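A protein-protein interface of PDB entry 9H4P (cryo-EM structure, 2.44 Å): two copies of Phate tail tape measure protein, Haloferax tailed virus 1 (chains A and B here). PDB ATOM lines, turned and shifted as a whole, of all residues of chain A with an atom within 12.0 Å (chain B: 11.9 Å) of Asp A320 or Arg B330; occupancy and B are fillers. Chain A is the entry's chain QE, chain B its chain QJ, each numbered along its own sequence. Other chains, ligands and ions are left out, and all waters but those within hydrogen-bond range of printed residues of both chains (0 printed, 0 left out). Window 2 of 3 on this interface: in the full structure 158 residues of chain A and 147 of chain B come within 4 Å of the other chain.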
ATOM      1  N   ASN A 316     -42.962  15.062  -1.503  1.00  0.00           N
ATOM      2  CA  ASN A 316     -41.856  14.581  -0.684  1.00  0.00           C
ATOM      3  C   ASN A 316     -41.312  13.260  -1.243  1.00  0.00           C
ATOM      4  O   ASN A 316     -41.366  12.235  -0.566  1.00  0.00           O
ATOM      5  CB  ASN A 316     -42.284  14.487   0.788  1.00  0.00           C
ATOM      6  CG  ASN A 316     -41.156  14.223   1.762  1.00  0.00           C
ATOM      7  OD1 ASN A 316     -41.253  13.333   2.600  1.00  0.00           O
ATOM      8  ND2 ASN A 316     -40.088  14.996   1.677  1.00  0.00           N
ATOM      9  N   ALA A 317     -40.785  13.291  -2.476  1.00  0.00           N
ATOM     10  CA  ALA A 317     -40.317  12.099  -3.180  1.00  0.00           C
ATOM     11  C   ALA A 317     -38.959  11.627  -2.650  1.00  0.00           C
ATOM     12  O   ALA A 317     -38.120  12.451  -2.295  1.00  0.00           O
ATOM     13  CB  ALA A 317     -40.275  12.368  -4.665  1.00  0.00           C
ATOM     14  N   THR A 318     -38.751  10.297  -2.605  1.00  0.00           N
ATOM     15  CA  THR A 318     -37.490   9.689  -2.181  1.00  0.00           C
ATOM     16  C   THR A 318     -37.035   8.611  -3.170  1.00  0.00           C
ATOM     17  O   THR A 318     -37.860   7.844  -3.664  1.00  0.00           O
ATOM     18  CB  THR A 318     -37.578   9.075  -0.773  1.00  0.00           C
ATOM     19  OG1 THR A 318     -38.420   7.923  -0.819  1.00  0.00           O
ATOM     20  CG2 THR A 318     -38.097  10.018   0.290  1.00  0.00           C
ATOM     21  N   ILE A 319     -35.719   8.554  -3.446  1.00  0.00           N
ATOM     22  CA  ILE A 319     -35.080   7.403  -4.079  1.00  0.00           C
ATOM     23  C   ILE A 319     -34.258   6.674  -3.016  1.00  0.00           C
ATOM     24  O   ILE A 319     -33.392   7.285  -2.391  1.00  0.00           O
ATOM     25  CB  ILE A 319     -34.204   7.805  -5.292  1.00  0.00           C
ATOM     26  CG1 ILE A 319     -35.047   8.360  -6.444  1.00  0.00           C
ATOM     27  CG2 ILE A 319     -33.321   6.647  -5.753  1.00  0.00           C
ATOM     28  CD1 ILE A 319     -34.249   8.982  -7.579  1.00  0.00           C
ATOM     29  N   ASP A 320     -34.545   5.379  -2.818  1.00  0.00           N
ATOM     30  CA  ASP A 320     -33.720   4.478  -2.019  1.00  0.00           C
ATOM     31  C   ASP A 320     -33.464   5.044  -0.616  1.00  0.00           C
ATOM     32  O   ASP A 320     -32.337   5.001  -0.123  1.00  0.00           O
ATOM     33  CB  ASP A 320     -32.455   4.081  -2.793  1.00  0.00           C
ATOM     34  CG  ASP A 320     -31.781   2.805  -2.320  1.00  0.00           C
ATOM     35  OD1 ASP A 320     -32.287   2.181  -1.369  1.00  0.00           O
ATOM     36  OD2 ASP A 320     -30.751   2.447  -2.910  1.00  0.00           O
ATOM     37  N   GLY A 321     -34.515   5.590   0.017  1.00  0.00           N
ATOM     38  CA  GLY A 321     -34.441   6.111   1.375  1.00  0.00           C
ATOM     39  C   GLY A 321     -34.003   7.576   1.500  1.00  0.00           C
ATOM     40  O   GLY A 321     -34.159   8.155   2.573  1.00  0.00           O
ATOM     41  N   ARG A 322     -33.457   8.171   0.425  1.00  0.00           N
ATOM     42  CA  ARG A 322     -32.965   9.548   0.421  1.00  0.00           C
ATOM     43  C   ARG A 322     -33.981  10.473  -0.253  1.00  0.00           C
ATOM     44  O   ARG A 322     -34.501  10.129  -1.309  1.00  0.00           O
ATOM     45  CB  ARG A 322     -31.632   9.633  -0.335  1.00  0.00           C
ATOM     46  CG  ARG A 322     -30.850  10.917  -0.096  1.00  0.00           C
ATOM     47  CD  ARG A 322     -29.962  11.356  -1.244  1.00  0.00           C
ATOM     48  NE  ARG A 322     -29.020  10.335  -1.680  1.00  0.00           N
ATOM     49  CZ  ARG A 322     -27.788  10.156  -1.213  1.00  0.00           C
ATOM     50  NH1 ARG A 322     -27.044   9.180  -1.698  1.00  0.00           N
ATOM     51  NH2 ARG A 322     -27.298  10.938  -0.271  1.00  0.00           N
ATOM     52  N   GLN A 323     -34.216  11.663   0.326  1.00  0.00           N
ATOM     53  CA  GLN A 323     -35.071  12.687  -0.271  1.00  0.00           C
ATOM     54  C   GLN A 323     -34.453  13.213  -1.571  1.00  0.00           C
ATOM     55  O   GLN A 323     -33.247  13.452  -1.626  1.00  0.00           O
ATOM     56  CB  GLN A 323     -35.305  13.843   0.707  1.00  0.00           C
ATOM     57  CG  GLN A 323     -36.022  13.445   1.992  1.00  0.00           C
ATOM     58  CD  GLN A 323     -36.553  14.609   2.793  1.00  0.00           C
ATOM     59  OE1 GLN A 323     -37.730  14.660   3.132  1.00  0.00           O
ATOM     60  NE2 GLN A 323     -35.687  15.557   3.106  1.00  0.00           N
ATOM     61  N   ILE A 324     -35.301  13.407  -2.600  1.00  0.00           N
ATOM     62  CA  ILE A 324     -34.908  13.969  -3.892  1.00  0.00           C
ATOM     63  C   ILE A 324     -35.635  15.286  -4.191  1.00  0.00           C
ATOM     64  O   ILE A 324     -35.280  15.964  -5.156  1.00  0.00           O
ATOM     65  CB  ILE A 324     -35.028  12.961  -5.062  1.00  0.00           C
ATOM     66  CG1 ILE A 324     -36.454  12.425  -5.241  1.00  0.00           C
ATOM     67  CG2 ILE A 324     -33.993  11.849  -4.941  1.00  0.00           C
ATOM     68  CD1 ILE A 324     -36.789  11.985  -6.654  1.00  0.00           C
ATOM     69  N   SER A 325     -36.651  15.643  -3.385  1.00  0.00           N
ATOM     70  CA  SER A 325     -37.238  16.978  -3.421  1.00  0.00           C
ATOM     71  C   SER A 325     -36.187  18.005  -3.006  1.00  0.00           C
ATOM     72  O   SER A 325     -35.523  17.816  -1.987  1.00  0.00           O
ATOM     73  CB  SER A 325     -38.446  17.069  -2.529  1.00  0.00           C
ATOM     74  OG  SER A 325     -39.489  16.241  -3.009  1.00  0.00           O
ATOM     75  N   ARG B 322     -28.851  17.063  -8.447  1.00  0.00           N
ATOM     76  CA  ARG B 322     -27.699  16.497  -7.755  1.00  0.00           C
ATOM     77  C   ARG B 322     -28.087  15.204  -7.040  1.00  0.00           C
ATOM     78  O   ARG B 322     -27.429  14.182  -7.229  1.00  0.00           O
ATOM     79  CB  ARG B 322     -27.073  17.494  -6.775  1.00  0.00           C
ATOM     80  CG  ARG B 322     -26.366  18.647  -7.468  1.00  0.00           C
ATOM     81  CD  ARG B 322     -25.608  19.571  -6.541  1.00  0.00           C
ATOM     82  NE  ARG B 322     -25.161  20.730  -7.304  1.00  0.00           N
ATOM     83  CZ  ARG B 322     -24.022  20.834  -7.986  1.00  0.00           C
ATOM     84  NH1 ARG B 322     -23.760  21.947  -8.647  1.00  0.00           N
ATOM     85  NH2 ARG B 322     -23.145  19.845  -8.010  1.00  0.00           N
ATOM     86  N   GLN B 323     -29.173  15.248  -6.255  1.00  0.00           N
ATOM     87  CA  GLN B 323     -29.558  14.102  -5.444  1.00  0.00           C
ATOM     88  C   GLN B 323     -30.153  12.958  -6.270  1.00  0.00           C
ATOM     89  O   GLN B 323     -30.029  11.812  -5.848  1.00  0.00           O
ATOM     90  CB  GLN B 323     -30.411  14.488  -4.233  1.00  0.00           C
ATOM     91  CG  GLN B 323     -29.714  15.423  -3.246  1.00  0.00           C
ATOM     92  CD  GLN B 323     -28.211  15.282  -3.149  1.00  0.00           C
ATOM     93  OE1 GLN B 323     -27.468  16.210  -3.451  1.00  0.00           O
ATOM     94  NE2 GLN B 323     -27.744  14.119  -2.729  1.00  0.00           N
ATOM     95  N   ILE B 324     -30.807  13.238  -7.410  1.00  0.00           N
ATOM     96  CA  ILE B 324     -31.181  12.159  -8.320  1.00  0.00           C
ATOM     97  C   ILE B 324     -29.914  11.485  -8.851  1.00  0.00           C
ATOM     98  O   ILE B 324     -29.759  10.277  -8.683  1.00  0.00           O
ATOM     99  CB  ILE B 324     -32.170  12.588  -9.433  1.00  0.00           C
ATOM    100  CG1 ILE B 324     -33.596  12.687  -8.876  1.00  0.00           C
ATOM    101  CG2 ILE B 324     -32.098  11.652 -10.642  1.00  0.00           C
ATOM    102  CD1 ILE B 324     -34.704  12.689  -9.912  1.00  0.00           C
ATOM    103  N   SER B 325     -29.003  12.274  -9.443  1.00  0.00           N
ATOM    104  CA  SER B 325     -27.834  11.730 -10.124  1.00  0.00           C
ATOM    105  C   SER B 325     -26.872  11.024  -9.163  1.00  0.00           C
ATOM    106  O   SER B 325     -26.218  10.062  -9.565  1.00  0.00           O
ATOM    107  CB  SER B 325     -27.139  12.754 -10.994  1.00  0.00           C
ATOM    108  OG  SER B 325     -26.616  13.814 -10.211  1.00  0.00           O
ATOM    109  N   GLU B 326     -26.809  11.481  -7.903  1.00  0.00           N
ATOM    110  CA  GLU B 326     -26.014  10.833  -6.865  1.00  0.00           C
ATOM    111  C   GLU B 326     -26.665   9.525  -6.401  1.00  0.00           C
ATOM    112  O   GLU B 326     -25.957   8.541  -6.175  1.00  0.00           O
ATOM    113  CB  GLU B 326     -25.757  11.793  -5.699  1.00  0.00           C
ATOM    114  CG  GLU B 326     -24.906  11.197  -4.590  1.00  0.00           C
ATOM    115  CD  GLU B 326     -24.340  12.214  -3.623  1.00  0.00           C
ATOM    116  OE1 GLU B 326     -25.064  13.155  -3.259  1.00  0.00           O
ATOM    117  OE2 GLU B 326     -23.172  12.065  -3.238  1.00  0.00           O
ATOM    118  N   SER B 327     -28.002   9.519  -6.260  1.00  0.00           N
ATOM    119  CA  SER B 327     -28.740   8.346  -5.804  1.00  0.00           C
ATOM    120  C   SER B 327     -28.749   7.221  -6.847  1.00  0.00           C
ATOM    121  O   SER B 327     -28.742   6.048  -6.470  1.00  0.00           O
ATOM    122  CB  SER B 327     -30.144   8.691  -5.361  1.00  0.00           C
ATOM    123  OG  SER B 327     -30.132   9.660  -4.322  1.00  0.00           O
ATOM    124  N   THR B 328     -28.768   7.572  -8.145  1.00  0.00           N
ATOM    125  CA  THR B 328     -28.875   6.574  -9.206  1.00  0.00           C
ATOM    126  C   THR B 328     -27.518   6.003  -9.633  1.00  0.00           C
ATOM    127  O   THR B 328     -27.501   5.065 -10.431  1.00  0.00           O
ATOM    128  CB  THR B 328     -29.688   7.056 -10.423  1.00  0.00           C
ATOM    129  OG1 THR B 328     -29.047   8.169 -11.051  1.00  0.00           O
ATOM    130  CG2 THR B 328     -31.134   7.375 -10.110  1.00  0.00           C
ATOM    131  N   GLY B 329     -26.397   6.547  -9.119  1.00  0.00           N
ATOM    132  CA  GLY B 329     -25.045   6.162  -9.520  1.00  0.00           C
ATOM    133  C   GLY B 329     -24.761   4.668  -9.363  1.00  0.00           C
ATOM    134  O   GLY B 329     -24.205   4.049 -10.271  1.00  0.00           O
ATOM    135  N   ARG B 330     -25.173   4.104  -8.214  1.00  0.00           N
ATOM    136  CA  ARG B 330     -25.044   2.687  -7.884  1.00  0.00           C
ATOM    137  C   ARG B 330     -25.740   1.781  -8.909  1.00  0.00           C
ATOM    138  O   ARG B 330     -25.338   0.630  -9.078  1.00  0.00           O
ATOM    139  CB  ARG B 330     -25.547   2.417  -6.460  1.00  0.00           C
ATOM    140  CG  ARG B 330     -27.035   2.679  -6.253  1.00  0.00           C
ATOM    141  CD  ARG B 330     -27.562   2.591  -4.833  1.00  0.00           C
ATOM    142  NE  ARG B 330     -26.919   3.579  -3.981  1.00  0.00           N
ATOM    143  CZ  ARG B 330     -27.269   3.897  -2.738  1.00  0.00           C
ATOM    144  NH1 ARG B 330     -26.580   4.814  -2.085  1.00  0.00           N
ATOM    145  NH2 ARG B 330     -28.297   3.318  -2.145  1.00  0.00           N
ATOM    146  N   TYR B 331     -26.769   2.317  -9.586  1.00  0.00           N
ATOM    147  CA  TYR B 331     -27.571   1.603 -10.574  1.00  0.00           C
ATOM    148  C   TYR B 331     -27.101   1.868 -12.013  1.00  0.00           C
ATOM    149  O   TYR B 331     -27.151   0.950 -12.831  1.00  0.00           O
ATOM    150  CB  TYR B 331     -29.061   1.894 -10.355  1.00  0.00           C
ATOM    151  CG  TYR B 331     -29.572   1.642  -8.954  1.00  0.00           C
ATOM    152  CD1 TYR B 331     -29.523   0.374  -8.388  1.00  0.00           C
ATOM    153  CD2 TYR B 331     -30.112   2.668  -8.189  1.00  0.00           C
ATOM    154  CE1 TYR B 331     -30.001   0.129  -7.108  1.00  0.00           C
ATOM    155  CE2 TYR B 331     -30.592   2.442  -6.906  1.00  0.00           C
ATOM    156  CZ  TYR B 331     -30.536   1.168  -6.364  1.00  0.00           C
ATOM    157  OH  TYR B 331     -31.001   0.937  -5.103  1.00  0.00           O
ATOM    158  N   ARG B 332     -26.644   3.096 -12.329  1.00  0.00           N
ATOM    159  CA  ARG B 332     -26.180   3.452 -13.671  1.00  0.00           C
ATOM    160  C   ARG B 332     -24.926   2.666 -14.074  1.00  0.00           C
ATOM    161  O   ARG B 332     -24.780   2.298 -15.241  1.00  0.00           O
ATOM    162  CB  ARG B 332     -25.887   4.951 -13.802  1.00  0.00           C
ATOM    163  CG  ARG B 332     -27.108   5.860 -13.742  1.00  0.00           C
ATOM    164  CD  ARG B 332     -26.843   7.244 -14.316  1.00  0.00           C
ATOM    165  NE  ARG B 332     -25.549   7.806 -13.927  1.00  0.00           N
ATOM    166  CZ  ARG B 332     -25.284   8.444 -12.787  1.00  0.00           C
ATOM    167  NH1 ARG B 332     -24.062   8.894 -12.557  1.00  0.00           N
ATOM    168  NH2 ARG B 332     -26.229   8.636 -11.882  1.00  0.00           N
ATOM    169  N   SER B 333     -24.031   2.427 -13.104  1.00  0.00           N
ATOM    170  CA  SER B 333     -22.770   1.721 -13.294  1.00  0.00           C
ATOM    171  C   SER B 333     -22.950   0.199 -13.318  1.00  0.00           C
ATOM    172  O   SER B 333     -22.031  -0.509 -13.730  1.00  0.00           O
ATOM    173  CB  SER B 333     -21.753   2.136 -12.246  1.00  0.00           C
ATOM    174  OG  SER B 333     -22.220   1.854 -10.932  1.00  0.00           O
ATOM    175  N   ASP B 334     -24.122  -0.296 -12.883  1.00  0.00           N
ATOM    176  CA  ASP B 334     -24.359  -1.715 -12.630  1.00  0.00           C
ATOM    177  C   ASP B 334     -24.185  -2.591 -13.878  1.00  0.00           C
ATOM    178  O   ASP B 334     -23.504  -3.615 -13.782  1.00  0.00           O
ATOM    179  CB  ASP B 334     -25.701  -1.942 -11.927  1.00  0.00           C
ATOM    180  CG  ASP B 334     -25.939  -3.380 -11.513  1.00  0.00           C
ATOM    181  OD1 ASP B 334     -25.042  -3.966 -10.877  1.00  0.00           O
ATOM    182  OD2 ASP B 334     -27.023  -3.897 -11.827  1.00  0.00           O
ATOM    183  N   PRO B 335     -24.790  -2.271 -15.060  1.00  0.00           N
ATOM    184  CA  PRO B 335     -24.634  -3.109 -16.255  1.00  0.00           C
ATOM    185  C   PRO B 335     -23.181  -3.315 -16.682  1.00  0.00           C
ATOM    186  O   PRO B 335     -22.835  -4.382 -17.185  1.00  0.00           O
ATOM    187  CB  PRO B 335     -25.412  -2.361 -17.355  1.00  0.00           C
ATOM    188  CG  PRO B 335     -26.409  -1.512 -16.592  1.00  0.00           C
ATOM    189  CD  PRO B 335     -25.674  -1.117 -15.328  1.00  0.00           C
ATOM    190  N   SER B 336     -22.344  -2.288 -16.469  1.00  0.00           N
ATOM    191  CA  SER B 336     -20.936  -2.342 -16.833  1.00  0.00           C
ATOM    192  C   SER B 336     -20.157  -3.246 -15.875  1.00  0.00           C
ATOM    193  O   SER B 336     -19.293  -3.995 -16.326  1.00  0.00           O
ATOM    194  CB  SER B 336     -20.334  -0.964 -16.971  1.00  0.00           C
ATOM    195  OG  SER B 336     -21.086  -0.167 -17.876  1.00  0.00           O
ATOM    196  N   ARG B 337     -20.487  -3.199 -14.572  1.00  0.00           N
ATOM    197  CA  ARG B 337     -19.926  -4.113 -13.583  1.00  0.00           C
ATOM    198  C   ARG B 337     -20.333  -5.557 -13.894  1.00  0.00           C
ATOM    199  O   ARG B 337     -19.500  -6.457 -13.783  1.00  0.00           O
ATOM    200  CB  ARG B 337     -20.266  -3.687 -12.149  1.00  0.00           C
ATOM    201  CG  ARG B 337     -19.228  -2.782 -11.497  1.00  0.00           C
ATOM    202  CD  ARG B 337     -18.903  -1.507 -12.261  1.00  0.00           C
ATOM    203  NE  ARG B 337     -18.030  -0.599 -11.529  1.00  0.00           N
ATOM    204  CZ  ARG B 337     -16.699  -0.626 -11.519  1.00  0.00           C
ATOM    205  NH1 ARG B 337     -16.041   0.266 -10.801  1.00  0.00           N
ATOM    206  NH2 ARG B 337     -16.024  -1.527 -12.212  1.00  0.00           N
ATOM    207  N   ARG B 338     -21.595  -5.757 -14.313  1.00  0.00           N
ATOM    208  CA  ARG B 338     -22.116  -7.047 -14.758  1.00  0.00           C
ATOM    209  C   ARG B 338     -21.343  -7.592 -15.965  1.00  0.00           C
ATOM    210  O   ARG B 338     -21.247  -8.809 -16.127  1.00  0.00           O
ATOM    211  CB  ARG B 338     -23.618  -6.944 -15.041  1.00  0.00           C
ATOM    212  CG  ARG B 338     -24.492  -7.166 -13.815  1.00  0.00           C
ATOM    213  CD  ARG B 338     -25.736  -6.300 -13.746  1.00  0.00           C
ATOM    214  NE  ARG B 338     -26.513  -6.291 -14.982  1.00  0.00           N
ATOM    215  CZ  ARG B 338     -27.486  -5.434 -15.285  1.00  0.00           C
ATOM    216  NH1 ARG B 338     -28.112  -5.531 -16.444  1.00  0.00           N
ATOM    217  NH2 ARG B 338     -27.844  -4.490 -14.432  1.00  0.00           N
ATOM    218  N   ARG B 339     -20.779  -6.690 -16.789  1.00  0.00           N
ATOM    219  CA  ARG B 339     -19.992  -7.041 -17.968  1.00  0.00           C
ATOM    220  C   ARG B 339     -18.481  -6.941 -17.719  1.00  0.00           C
ATOM    221  O   ARG B 339     -17.703  -6.893 -18.673  1.00  0.00           O
ATOM    222  CB  ARG B 339     -20.460  -6.223 -19.176  1.00  0.00           C
ATOM    223  CG  ARG B 339     -21.851  -6.617 -19.647  1.00  0.00           C
ATOM    224  CD  ARG B 339     -22.402  -5.620 -20.634  1.00  0.00           C
ATOM    225  NE  ARG B 339     -21.901  -5.782 -21.992  1.00  0.00           N
ATOM    226  CZ  ARG B 339     -22.277  -5.027 -23.018  1.00  0.00           C
ATOM    227  NH1 ARG B 339     -21.784  -5.245 -24.224  1.00  0.00           N
ATOM    228  NH2 ARG B 339     -23.154  -4.055 -22.842  1.00  0.00           N
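The side-chain carboxylate of Asp A320 is in hydrogen-bond range of the side-chain hydroxyl of Tyr B331 (2.7 Å).
NH2 of Arg B330 is in salt-bridge range of OD2 of Asp A320 (2.7 Å).
The side-chain hydroxyl of Ser B327 lies within hydrogen-bond range of the guanidinium group of Arg A322 (2.9 Å).
The side-chain amide oxygen (OE1) of Gln A323 lies within hydrogen-bond range of the side-chain amide nitrogen (ND2) of Asn A316, at 2.8 Å.
The side-chain hydroxyl (OG) of Ser B327 sits at hydrogen-bond distance from the backbone carbonyl oxygen (O) of Gln B323, at 2.6 Å.
O of Ala A317 is in hydrogen-bond range of N of Ile A324 (3.0 Å).
NE2 of Gln B323 lies within hydrogen-bond range of OE1 of Glu B326 (2.9 Å).
OG1 of Thr B328 lies within hydrogen-bond range of O of Ile B324 (3.2 Å).
Ile A319 touches Ile B324.
Ser B327 touches Ile A319 (CB to CG2, 3.8 Å).
CD of Arg A322 touches NE2 of Gln B323, 3.8 Å away.
Gln A323 touches Gln B323.
Ile B324 touches Ile A324.
Asp A320 touches just these residues of chain B: Arg B330 (2.7 Å) and Tyr B331 (2.7 Å).
Ile A319 touches two residues of chain B.
No residue of chain B comes within 4 Å of Gly A321.
Arg A322 touches just these residues of chain B: Gln B323 and Ser B327.
Ser B327 touches just these residues of chain A: Ile A319 (3.8 Å) and Arg A322 (2.9 Å).
No residue of chain A comes within 4 Å of Thr B328.
Tyr B331 touches just one residue of chain A: Asp A320 (2.7 Å).
No residue of chain A comes within 4 Å of Arg B332.
No residue of chain A comes within 4 Å of Asp B334.
Of the printed residues of chain B, Gln A323 touches Gln B323.
Printed residues of chain A within 4 Å of Ile B324: Ile A319 and Ile A324.
Of the printed residues of chain A, Gln B323 touches Arg A322 and Gln A323.
The nearest residue of chain A that does not touch Arg B330 is Arg A322 (4.4 Å).
Printed residues of chain A that touch a printed residue of chain B: Ile A319, Asp A320, Arg A322, Gln A323 and Ile A324.
Printed residues of chain B that touch a printed residue of chain A: Gln B323, Ile B324, Ser B327, Arg B330 and Tyr B331.
Hydrophobic or aromatic side chains of chain B within 4 Å of the printed part of chain A: Ile B324 and Tyr B331.
Among the printed residues, 8 pairs touch across the chains.
Arg A322 touches Gln B323, but with the chains exchanged Gln A323 does not touch Arg B322 (7.7 Å).
Gln A323 touches its own counterpart, Gln B323.
Ile B324 touches its own counterpart, Ile A324.
4 positions are printed for both chains.
Of the 8 pairs that touch across the chains among the printed residues, 2 have their exchanged pair printed and touching as well.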
